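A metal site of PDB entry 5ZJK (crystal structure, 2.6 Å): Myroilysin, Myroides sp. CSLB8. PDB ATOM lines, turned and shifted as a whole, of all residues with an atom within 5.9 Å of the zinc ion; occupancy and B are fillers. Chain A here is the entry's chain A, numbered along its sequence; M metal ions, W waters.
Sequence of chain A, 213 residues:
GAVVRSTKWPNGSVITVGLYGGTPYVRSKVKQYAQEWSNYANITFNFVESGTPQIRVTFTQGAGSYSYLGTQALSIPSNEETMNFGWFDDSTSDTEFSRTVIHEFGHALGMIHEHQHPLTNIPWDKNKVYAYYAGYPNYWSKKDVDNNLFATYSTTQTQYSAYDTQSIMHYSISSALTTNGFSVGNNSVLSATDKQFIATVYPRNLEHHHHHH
Water W1 bridges O of Ser 65 and OH of Tyr 171.
Tyr 171 touches the zinc ion (OH to ZN, 3.996 Å). The nearest printed residue that does not touch the zinc ion is Glu 104 (4.02 Å).
The side-chain hydroxyl (OH) of Tyr 171 sits close to a ring nitrogen (NE2) of His 113 (3.3 Å).
The zinc ion is bound by a ring nitrogen (NE2) of His 113 (2.2 Å), a ring nitrogen (NE2) of His 107 (2.2 Å) and a ring nitrogen (NE2) of His 103 (2.2 Å).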
ATOM      1  N   SER A  65      15.298  19.104  -9.219  1.00  0.00           N
ATOM      2  CA  SER A  65      16.513  18.299  -9.314  1.00  0.00           C
ATOM      3  C   SER A  65      17.173  18.164  -7.951  1.00  0.00           C
ATOM      4  O   SER A  65      17.320  19.153  -7.234  1.00  0.00           O
ATOM      5  CB  SER A  65      17.489  18.907 -10.328  1.00  0.00           C
ATOM      6  OG  SER A  65      16.962  18.866 -11.636  1.00  0.00           O
ATOM      7  N   HIS A 103      26.603  18.653 -10.710  1.00  0.00           N
ATOM      8  CA  HIS A 103      26.207  19.043  -9.409  1.00  0.00           C
ATOM      9  C   HIS A 103      25.402  17.978  -8.620  1.00  0.00           C
ATOM     10  O   HIS A 103      25.584  17.838  -7.448  1.00  0.00           O
ATOM     11  CB  HIS A 103      25.490  20.331  -9.564  1.00  0.00           C
ATOM     12  CG  HIS A 103      24.892  20.885  -8.315  1.00  0.00           C
ATOM     13  ND1 HIS A 103      25.385  21.996  -7.701  1.00  0.00           N
ATOM     14  CD2 HIS A 103      23.831  20.507  -7.607  1.00  0.00           C
ATOM     15  CE1 HIS A 103      24.648  22.275  -6.660  1.00  0.00           C
ATOM     16  NE2 HIS A 103      23.700  21.381  -6.570  1.00  0.00           N
ATOM     17  N   GLU A 104      24.534  17.212  -9.249  1.00  0.00           N
ATOM     18  CA  GLU A 104      23.809  16.315  -8.510  1.00  0.00           C
ATOM     19  C   GLU A 104      24.739  15.030  -8.248  1.00  0.00           C
ATOM     20  O   GLU A 104      24.627  14.410  -7.292  1.00  0.00           O
ATOM     21  CB  GLU A 104      22.548  15.872  -9.263  1.00  0.00           C
ATOM     22  CG  GLU A 104      21.549  16.984  -9.496  1.00  0.00           C
ATOM     23  CD  GLU A 104      21.079  17.636  -8.207  1.00  0.00           C
ATOM     24  OE1 GLU A 104      20.866  16.907  -7.224  1.00  0.00           O
ATOM     25  OE2 GLU A 104      20.921  18.872  -8.192  1.00  0.00           O
ATOM     26  N   HIS A 107      26.578  15.694  -5.217  1.00  0.00           N
ATOM     27  CA  HIS A 107      25.874  15.334  -4.037  1.00  0.00           C
ATOM     28  C   HIS A 107      25.988  13.841  -3.781  1.00  0.00           C
ATOM     29  O   HIS A 107      26.122  13.419  -2.672  1.00  0.00           O
ATOM     30  CB  HIS A 107      24.438  15.661  -4.173  1.00  0.00           C
ATOM     31  CG  HIS A 107      24.108  17.073  -3.869  1.00  0.00           C
ATOM     32  ND1 HIS A 107      24.700  17.759  -2.857  1.00  0.00           N
ATOM     33  CD2 HIS A 107      23.258  17.913  -4.449  1.00  0.00           C
ATOM     34  CE1 HIS A 107      24.199  18.955  -2.793  1.00  0.00           C
ATOM     35  NE2 HIS A 107      23.325  19.081  -3.761  1.00  0.00           N
ATOM     36  N   HIS A 113      26.156  21.817  -0.380  1.00  0.00           N
ATOM     37  CA  HIS A 113      26.066  23.054  -1.104  1.00  0.00           C
ATOM     38  C   HIS A 113      27.123  23.970  -0.615  1.00  0.00           C
ATOM     39  O   HIS A 113      27.259  24.101   0.555  1.00  0.00           O
ATOM     40  CB  HIS A 113      24.741  23.695  -0.897  1.00  0.00           C
ATOM     41  CG  HIS A 113      23.659  23.082  -1.698  1.00  0.00           C
ATOM     42  ND1 HIS A 113      22.359  23.051  -1.283  1.00  0.00           N
ATOM     43  CD2 HIS A 113      23.683  22.487  -2.893  1.00  0.00           C
ATOM     44  CE1 HIS A 113      21.636  22.425  -2.170  1.00  0.00           C
ATOM     45  NE2 HIS A 113      22.416  22.082  -3.169  1.00  0.00           N
ATOM     46  N   MET A 169      29.065  23.232  -6.831  1.00  0.00           N
ATOM     47  CA  MET A 169      28.062  23.035  -5.787  1.00  0.00           C
ATOM     48  C   MET A 169      27.563  24.349  -5.199  1.00  0.00           C
ATOM     49  O   MET A 169      26.839  24.354  -4.214  1.00  0.00           O
ATOM     50  CB  MET A 169      28.634  22.171  -4.667  1.00  0.00           C
ATOM     51  CG  MET A 169      29.264  20.886  -5.161  1.00  0.00           C
ATOM     52  SD  MET A 169      28.106  19.875  -6.105  1.00  0.00           S
ATOM     53  CE  MET A 169      26.800  19.657  -4.902  1.00  0.00           C
ATOM     54  N   TYR A 171      25.330  27.672  -5.496  1.00  0.00           N
ATOM     55  CA  TYR A 171      24.233  28.256  -6.185  1.00  0.00           C
ATOM     56  C   TYR A 171      24.549  29.677  -6.556  1.00  0.00           C
ATOM     57  O   TYR A 171      25.238  30.349  -5.885  1.00  0.00           O
ATOM     58  CB  TYR A 171      23.045  28.358  -5.232  1.00  0.00           C
ATOM     59  CG  TYR A 171      22.203  27.148  -5.038  1.00  0.00           C
ATOM     60  CD1 TYR A 171      22.465  25.976  -5.688  1.00  0.00           C
ATOM     61  CD2 TYR A 171      21.164  27.171  -4.172  1.00  0.00           C
ATOM     62  CE1 TYR A 171      21.713  24.877  -5.479  1.00  0.00           C
ATOM     63  CE2 TYR A 171      20.381  26.073  -3.961  1.00  0.00           C
ATOM     64  CZ  TYR A 171      20.676  24.925  -4.641  1.00  0.00           C
ATOM     65  OH  TYR A 171      19.887  23.840  -4.469  1.00  0.00           O
HETATM   66 ZN    ZN M   1      22.335  20.713  -4.912  1.00  0.00          ZN
HETATM   67  O   HOH W   1      19.335  20.929  -5.681  1.00  0.00           O
